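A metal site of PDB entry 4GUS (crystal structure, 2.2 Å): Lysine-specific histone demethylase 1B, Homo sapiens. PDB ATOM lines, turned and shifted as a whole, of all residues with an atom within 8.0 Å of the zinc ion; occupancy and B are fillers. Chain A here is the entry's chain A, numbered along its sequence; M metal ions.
The backbone NH (N) of Ala 28 sits close to the side-chain sulfur (SG) of Cys 46. The backbone NH (N) of Glu 48 sits close to the side-chain sulfur (SG) of Cys 46 (3.6 Å). SG of Cys 49 lies close to N of Ala 23 (3.3 Å). The backbone NH (N) of Ser 24 sits close to the side-chain sulfur (SG) of Cys 49, at 3.5 Å. SG of Cys 27 lies close to N of Lys 29. The side-chain sulfur (SG) of Cys 19 sits close to the backbone NH (N) of Ser 22, at 3.8 Å. The backbone NH (N) of Ala 21 lies close to the side-chain sulfur (SG) of Cys 19 (3.5 Å). N of Cys 19 is in hydrogen-bond range of O of Lys 29 (3.0 Å).
Residues that only touch the zinc ion: Ala 28.
The zinc ion is bound by the side-chain sulfur (SG) of Cys 46, 2.1 Å away. The zinc ion is bound by SG of Cys 49, at 2.3 Å. The zinc ion is bound by SG of Cys 27 (2.3 Å). SG of Cys 19 binds the zinc ion (2.4 Å). The zinc ion has four donor atoms within binding distance.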
ATOM      1  N   VAL A  18      -8.075   9.742  18.543  1.00  0.00           N
ATOM      2  CA  VAL A  18      -8.930  10.913  18.372  1.00  0.00           C
ATOM      3  C   VAL A  18     -10.183  10.515  17.593  1.00  0.00           C
ATOM      4  O   VAL A  18     -10.166   9.540  16.841  1.00  0.00           O
ATOM      5  CB  VAL A  18      -8.208  12.087  17.654  1.00  0.00           C
ATOM      6  CG1 VAL A  18      -6.970  12.509  18.442  1.00  0.00           C
ATOM      7  CG2 VAL A  18      -7.837  11.717  16.220  1.00  0.00           C
ATOM      8  N   CYS A  19     -11.281  11.234  17.795  1.00  0.00           N
ATOM      9  CA  CYS A  19     -12.506  10.926  17.079  1.00  0.00           C
ATOM     10  C   CYS A  19     -12.480  11.680  15.752  1.00  0.00           C
ATOM     11  O   CYS A  19     -12.245  12.887  15.738  1.00  0.00           O
ATOM     12  CB  CYS A  19     -13.749  11.334  17.870  1.00  0.00           C
ATOM     13  SG  CYS A  19     -15.313  10.743  17.150  1.00  0.00           S
ATOM     14  N   PHE A  20     -12.713  10.971  14.651  1.00  0.00           N
ATOM     15  CA  PHE A  20     -12.770  11.637  13.346  1.00  0.00           C
ATOM     16  C   PHE A  20     -14.185  12.144  13.062  1.00  0.00           C
ATOM     17  O   PHE A  20     -14.371  13.029  12.228  1.00  0.00           O
ATOM     18  CB  PHE A  20     -12.324  10.689  12.226  1.00  0.00           C
ATOM     19  CG  PHE A  20     -13.199   9.469  12.094  1.00  0.00           C
ATOM     20  CD1 PHE A  20     -12.767   8.249  12.574  1.00  0.00           C
ATOM     21  CD2 PHE A  20     -14.449   9.554  11.487  1.00  0.00           C
ATOM     22  CE1 PHE A  20     -13.568   7.135  12.461  1.00  0.00           C
ATOM     23  CE2 PHE A  20     -15.246   8.461  11.380  1.00  0.00           C
ATOM     24  CZ  PHE A  20     -14.814   7.241  11.860  1.00  0.00           C
ATOM     25  N   ALA A  21     -15.172  11.548  13.717  1.00  0.00           N
ATOM     26  CA  ALA A  21     -16.582  11.882  13.500  1.00  0.00           C
ATOM     27  C   ALA A  21     -16.923  13.314  13.888  1.00  0.00           C
ATOM     28  O   ALA A  21     -17.407  14.085  13.055  1.00  0.00           O
ATOM     29  CB  ALA A  21     -17.478  10.922  14.254  1.00  0.00           C
ATOM     30  N   SER A  22     -16.660  13.650  15.155  1.00  0.00           N
ATOM     31  CA  SER A  22     -17.050  14.939  15.733  1.00  0.00           C
ATOM     32  C   SER A  22     -18.482  15.302  15.381  1.00  0.00           C
ATOM     33  O   SER A  22     -18.774  16.432  15.009  1.00  0.00           O
ATOM     34  CB  SER A  22     -16.070  16.056  15.329  1.00  0.00           C
ATOM     35  OG  SER A  22     -15.757  16.012  13.951  1.00  0.00           O
ATOM     36  N   ALA A  23     -19.368  14.318  15.515  1.00  0.00           N
ATOM     37  CA  ALA A  23     -20.771  14.439  15.154  1.00  0.00           C
ATOM     38  C   ALA A  23     -21.573  14.914  16.345  1.00  0.00           C
ATOM     39  O   ALA A  23     -22.250  15.936  16.272  1.00  0.00           O
ATOM     40  CB  ALA A  23     -21.306  13.084  14.657  1.00  0.00           C
ATOM     41  N   SER A  24     -21.502  14.154  17.434  1.00  0.00           N
ATOM     42  CA  SER A  24     -22.220  14.463  18.674  1.00  0.00           C
ATOM     43  C   SER A  24     -21.721  15.747  19.314  1.00  0.00           C
ATOM     44  O   SER A  24     -20.528  16.071  19.268  1.00  0.00           O
ATOM     45  CB  SER A  24     -22.075  13.319  19.682  1.00  0.00           C
ATOM     46  OG  SER A  24     -22.673  13.672  20.920  1.00  0.00           O
ATOM     47  N   GLU A  25     -22.652  16.482  19.933  1.00  0.00           N
ATOM     48  CA  GLU A  25     -22.298  17.650  20.728  1.00  0.00           C
ATOM     49  C   GLU A  25     -21.376  17.260  21.880  1.00  0.00           C
ATOM     50  O   GLU A  25     -20.547  18.059  22.306  1.00  0.00           O
ATOM     51  CB  GLU A  25     -23.549  18.369  21.254  1.00  0.00           C
ATOM     52  CG  GLU A  25     -24.124  19.347  20.253  1.00  0.00           C
ATOM     53  CD  GLU A  25     -23.126  20.424  19.873  1.00  0.00           C
ATOM     54  OE1 GLU A  25     -22.394  20.895  20.776  1.00  0.00           O
ATOM     55  OE2 GLU A  25     -23.058  20.786  18.681  1.00  0.00           O
ATOM     56  N   ARG A  26     -21.510  16.010  22.345  1.00  0.00           N
ATOM     57  CA  ARG A  26     -20.663  15.469  23.404  1.00  0.00           C
ATOM     58  C   ARG A  26     -19.461  14.642  22.926  1.00  0.00           C
ATOM     59  O   ARG A  26     -18.985  13.760  23.654  1.00  0.00           O
ATOM     60  CB  ARG A  26     -21.509  14.571  24.303  1.00  0.00           C
ATOM     61  CG  ARG A  26     -22.267  15.316  25.379  1.00  0.00           C
ATOM     62  CD  ARG A  26     -21.462  15.418  26.667  1.00  0.00           C
ATOM     63  NE  ARG A  26     -22.084  16.387  27.553  1.00  0.00           N
ATOM     64  CZ  ARG A  26     -23.177  16.143  28.259  1.00  0.00           C
ATOM     65  NH1 ARG A  26     -23.758  14.936  28.194  1.00  0.00           N
ATOM     66  NH2 ARG A  26     -23.691  17.086  29.032  1.00  0.00           N
ATOM     67  N   CYS A  27     -18.968  14.914  21.717  1.00  0.00           N
ATOM     68  CA  CYS A  27     -17.857  14.154  21.144  1.00  0.00           C
ATOM     69  C   CYS A  27     -16.642  14.155  22.077  1.00  0.00           C
ATOM     70  O   CYS A  27     -16.242  15.209  22.569  1.00  0.00           O
ATOM     71  CB  CYS A  27     -17.482  14.716  19.760  1.00  0.00           C
ATOM     72  SG  CYS A  27     -16.010  13.968  18.961  1.00  0.00           S
ATOM     73  N   ALA A  28     -16.064  12.982  22.310  1.00  0.00           N
ATOM     74  CA  ALA A  28     -14.899  12.876  23.188  1.00  0.00           C
ATOM     75  C   ALA A  28     -13.676  13.627  22.653  1.00  0.00           C
ATOM     76  O   ALA A  28     -12.760  13.945  23.416  1.00  0.00           O
ATOM     77  CB  ALA A  28     -14.569  11.415  23.459  1.00  0.00           C
ATOM     78  N   LYS A  29     -13.662  13.925  21.350  1.00  0.00           N
ATOM     79  CA  LYS A  29     -12.506  14.540  20.696  1.00  0.00           C
ATOM     80  C   LYS A  29     -11.247  13.691  20.903  1.00  0.00           C
ATOM     81  O   LYS A  29     -11.214  12.524  20.510  1.00  0.00           O
ATOM     82  CB  LYS A  29     -12.275  15.969  21.207  1.00  0.00           C
ATOM     83  CG  LYS A  29     -13.464  16.888  21.035  1.00  0.00           C
ATOM     84  CD  LYS A  29     -13.640  17.309  19.599  1.00  0.00           C
ATOM     85  CE  LYS A  29     -14.731  18.359  19.437  1.00  0.00           C
ATOM     86  NZ  LYS A  29     -14.716  18.974  18.072  1.00  0.00           N
ATOM     87  N   ASN A  30     -10.237  14.280  21.540  1.00  0.00           N
ATOM     88  CA  ASN A  30      -9.029  13.551  21.916  1.00  0.00           C
ATOM     89  C   ASN A  30      -9.066  13.069  23.368  1.00  0.00           C
ATOM     90  O   ASN A  30      -8.021  12.824  23.963  1.00  0.00           O
ATOM     91  CB  ASN A  30      -7.809  14.438  21.723  1.00  0.00           C
ATOM     92  CG  ASN A  30      -7.813  15.642  22.664  1.00  0.00           C
ATOM     93  OD1 ASN A  30      -8.800  15.913  23.348  1.00  0.00           O
ATOM     94  ND2 ASN A  30      -6.700  16.370  22.696  1.00  0.00           N
ATOM     95  N   THR A  33     -13.782   8.371  26.729  1.00  0.00           N
ATOM     96  CA  THR A  33     -15.090   7.843  26.366  1.00  0.00           C
ATOM     97  C   THR A  33     -15.220   6.421  26.899  1.00  0.00           C
ATOM     98  O   THR A  33     -14.216   5.735  27.137  1.00  0.00           O
ATOM     99  CB  THR A  33     -15.357   7.927  24.816  1.00  0.00           C
ATOM    100  OG1 THR A  33     -16.633   7.343  24.507  1.00  0.00           O
ATOM    101  CG2 THR A  33     -14.272   7.210  24.015  1.00  0.00           C
ATOM    102  N   TRP A  36     -13.769   3.411  22.616  1.00  0.00           N
ATOM    103  CA  TRP A  36     -13.226   3.903  21.362  1.00  0.00           C
ATOM    104  C   TRP A  36     -13.448   2.842  20.303  1.00  0.00           C
ATOM    105  O   TRP A  36     -13.017   1.693  20.451  1.00  0.00           O
ATOM    106  CB  TRP A  36     -11.744   4.192  21.506  1.00  0.00           C
ATOM    107  CG  TRP A  36     -11.466   5.516  22.085  1.00  0.00           C
ATOM    108  CD1 TRP A  36     -10.973   5.784  23.322  1.00  0.00           C
ATOM    109  CD2 TRP A  36     -11.674   6.778  21.445  1.00  0.00           C
ATOM    110  NE1 TRP A  36     -10.850   7.136  23.507  1.00  0.00           N
ATOM    111  CE2 TRP A  36     -11.271   7.780  22.369  1.00  0.00           C
ATOM    112  CE3 TRP A  36     -12.149   7.182  20.191  1.00  0.00           C
ATOM    113  CZ2 TRP A  36     -11.332   9.149  22.073  1.00  0.00           C
ATOM    114  CZ3 TRP A  36     -12.211   8.541  19.897  1.00  0.00           C
ATOM    115  CH2 TRP A  36     -11.801   9.504  20.836  1.00  0.00           C
ATOM    116  N   HIS A  44     -10.399   6.274  14.693  1.00  0.00           N
ATOM    117  CA  HIS A  44     -11.324   5.801  15.718  1.00  0.00           C
ATOM    118  C   HIS A  44     -12.459   6.800  15.854  1.00  0.00           C
ATOM    119  O   HIS A  44     -12.347   7.946  15.420  1.00  0.00           O
ATOM    120  CB  HIS A  44     -10.602   5.648  17.064  1.00  0.00           C
ATOM    121  CG  HIS A  44      -9.339   4.857  16.982  1.00  0.00           C
ATOM    122  ND1 HIS A  44      -8.187   5.354  16.410  1.00  0.00           N
ATOM    123  CD2 HIS A  44      -9.053   3.574  17.349  1.00  0.00           C
ATOM    124  CE1 HIS A  44      -7.248   4.421  16.432  1.00  0.00           C
ATOM    125  NE2 HIS A  44      -7.747   3.341  16.992  1.00  0.00           N
ATOM    126  N   PHE A  45     -13.555   6.361  16.446  1.00  0.00           N
ATOM    127  CA  PHE A  45     -14.609   7.296  16.791  1.00  0.00           C
ATOM    128  C   PHE A  45     -15.156   6.985  18.184  1.00  0.00           C
ATOM    129  O   PHE A  45     -15.101   5.830  18.634  1.00  0.00           O
ATOM    130  CB  PHE A  45     -15.708   7.355  15.709  1.00  0.00           C
ATOM    131  CG  PHE A  45     -16.386   6.052  15.443  1.00  0.00           C
ATOM    132  CD1 PHE A  45     -17.592   5.743  16.049  1.00  0.00           C
ATOM    133  CD2 PHE A  45     -15.839   5.124  14.556  1.00  0.00           C
ATOM    134  CE1 PHE A  45     -18.241   4.530  15.793  1.00  0.00           C
ATOM    135  CE2 PHE A  45     -16.476   3.921  14.306  1.00  0.00           C
ATOM    136  CZ  PHE A  45     -17.678   3.623  14.920  1.00  0.00           C
ATOM    137  N   CYS A  46     -15.642   8.019  18.864  1.00  0.00           N
ATOM    138  CA  CYS A  46     -16.039   7.905  20.266  1.00  0.00           C
ATOM    139  C   CYS A  46     -17.437   7.325  20.387  1.00  0.00           C
ATOM    140  O   CYS A  46     -18.225   7.410  19.450  1.00  0.00           O
ATOM    141  CB  CYS A  46     -16.015   9.279  20.935  1.00  0.00           C
ATOM    142  SG  CYS A  46     -17.260  10.403  20.288  1.00  0.00           S
ATOM    143  N   ASN A  47     -17.739   6.765  21.558  1.00  0.00           N
ATOM    144  CA  ASN A  47     -19.064   6.203  21.826  1.00  0.00           C
ATOM    145  C   ASN A  47     -20.201   7.211  21.733  1.00  0.00           C
ATOM    146  O   ASN A  47     -21.352   6.850  21.496  1.00  0.00           O
ATOM    147  CB  ASN A  47     -19.075   5.504  23.182  1.00  0.00           C
ATOM    148  CG  ASN A  47     -20.352   4.724  23.412  1.00  0.00           C
ATOM    149  OD1 ASN A  47     -20.540   3.641  22.868  1.00  0.00           O
ATOM    150  ND2 ASN A  47     -21.233   5.266  24.247  1.00  0.00           N
ATOM    151  N   GLU A  48     -19.881   8.497  21.925  1.00  0.00           N
ATOM    152  CA  GLU A  48     -20.897   9.542  21.789  1.00  0.00           C
ATOM    153  C   GLU A  48     -21.308   9.712  20.319  1.00  0.00           C
ATOM    154  O   GLU A  48     -22.478   9.969  20.030  1.00  0.00           O
ATOM    155  CB  GLU A  48     -20.421  10.871  22.375  1.00  0.00           C
ATOM    156  CG  GLU A  48     -20.865  11.090  23.828  1.00  0.00           C
ATOM    157  CD  GLU A  48     -22.382  11.292  23.977  1.00  0.00           C
ATOM    158  OE1 GLU A  48     -22.972  10.670  24.889  1.00  0.00           O
ATOM    159  OE2 GLU A  48     -22.989  12.070  23.201  1.00  0.00           O
ATOM    160  N   CYS A  49     -20.360   9.579  19.415  1.00  0.00           N
ATOM    161  CA  CYS A  49     -20.656   9.703  18.000  1.00  0.00           C
ATOM    162  C   CYS A  49     -21.283   8.430  17.438  1.00  0.00           C
ATOM    163  O   CYS A  49     -22.083   8.478  16.520  1.00  0.00           O
ATOM    164  CB  CYS A  49     -19.406  10.097  17.226  1.00  0.00           C
ATOM    165  SG  CYS A  49     -18.905  11.770  17.587  1.00  0.00           S
ATOM    166  N   PHE A  50     -20.891   7.293  18.007  1.00  0.00           N
ATOM    167  CA  PHE A  50     -21.552   6.029  17.742  1.00  0.00           C
ATOM    168  C   PHE A  50     -23.056   6.187  17.998  1.00  0.00           C
ATOM    169  O   PHE A  50     -23.871   5.917  17.123  1.00  0.00           O
ATOM    170  CB  PHE A  50     -20.961   4.950  18.651  1.00  0.00           C
ATOM    171  CG  PHE A  50     -21.568   3.584  18.483  1.00  0.00           C
ATOM    172  CD1 PHE A  50     -21.005   2.659  17.623  1.00  0.00           C
ATOM    173  CD2 PHE A  50     -22.685   3.216  19.224  1.00  0.00           C
ATOM    174  CE1 PHE A  50     -21.558   1.395  17.489  1.00  0.00           C
ATOM    175  CE2 PHE A  50     -23.240   1.950  19.080  1.00  0.00           C
ATOM    176  CZ  PHE A  50     -22.674   1.045  18.216  1.00  0.00           C
ATOM    177  N   HIS A  52     -24.872   8.922  18.415  1.00  0.00           N
ATOM    178  CA  HIS A  52     -25.440   9.956  17.559  1.00  0.00           C
ATOM    179  C   HIS A  52     -26.150   9.353  16.350  1.00  0.00           C
ATOM    180  O   HIS A  52     -27.281   9.735  16.043  1.00  0.00           O
ATOM    181  CB  HIS A  52     -24.330  10.913  17.110  1.00  0.00           C
ATOM    182  CG  HIS A  52     -24.805  12.008  16.203  1.00  0.00           C
ATOM    183  ND1 HIS A  52     -25.260  13.224  16.672  1.00  0.00           N
ATOM    184  CD2 HIS A  52     -24.872  12.071  14.851  1.00  0.00           C
ATOM    185  CE1 HIS A  52     -25.586  13.990  15.649  1.00  0.00           C
ATOM    186  NE2 HIS A  52     -25.371  13.311  14.538  1.00  0.00           N
ATOM    187  N   MET A  85     -19.608   4.587   9.040  1.00  0.00           N
ATOM    188  CA  MET A  85     -18.534   5.567   9.238  1.00  0.00           C
ATOM    189  C   MET A  85     -17.524   5.534   8.087  1.00  0.00           C
ATOM    190  O   MET A  85     -17.102   6.582   7.580  1.00  0.00           O
ATOM    191  CB  MET A  85     -17.814   5.300  10.572  1.00  0.00           C
ATOM    192  CG  MET A  85     -18.676   5.476  11.823  1.00  0.00           C
ATOM    193  SD  MET A  85     -19.440   7.108  11.880  1.00  0.00           S
ATOM    194  CE  MET A  85     -18.223   8.067  12.724  1.00  0.00           C
HETATM  195 ZN    ZN M   1     -16.844  11.786  18.713  1.00  0.00          ZN
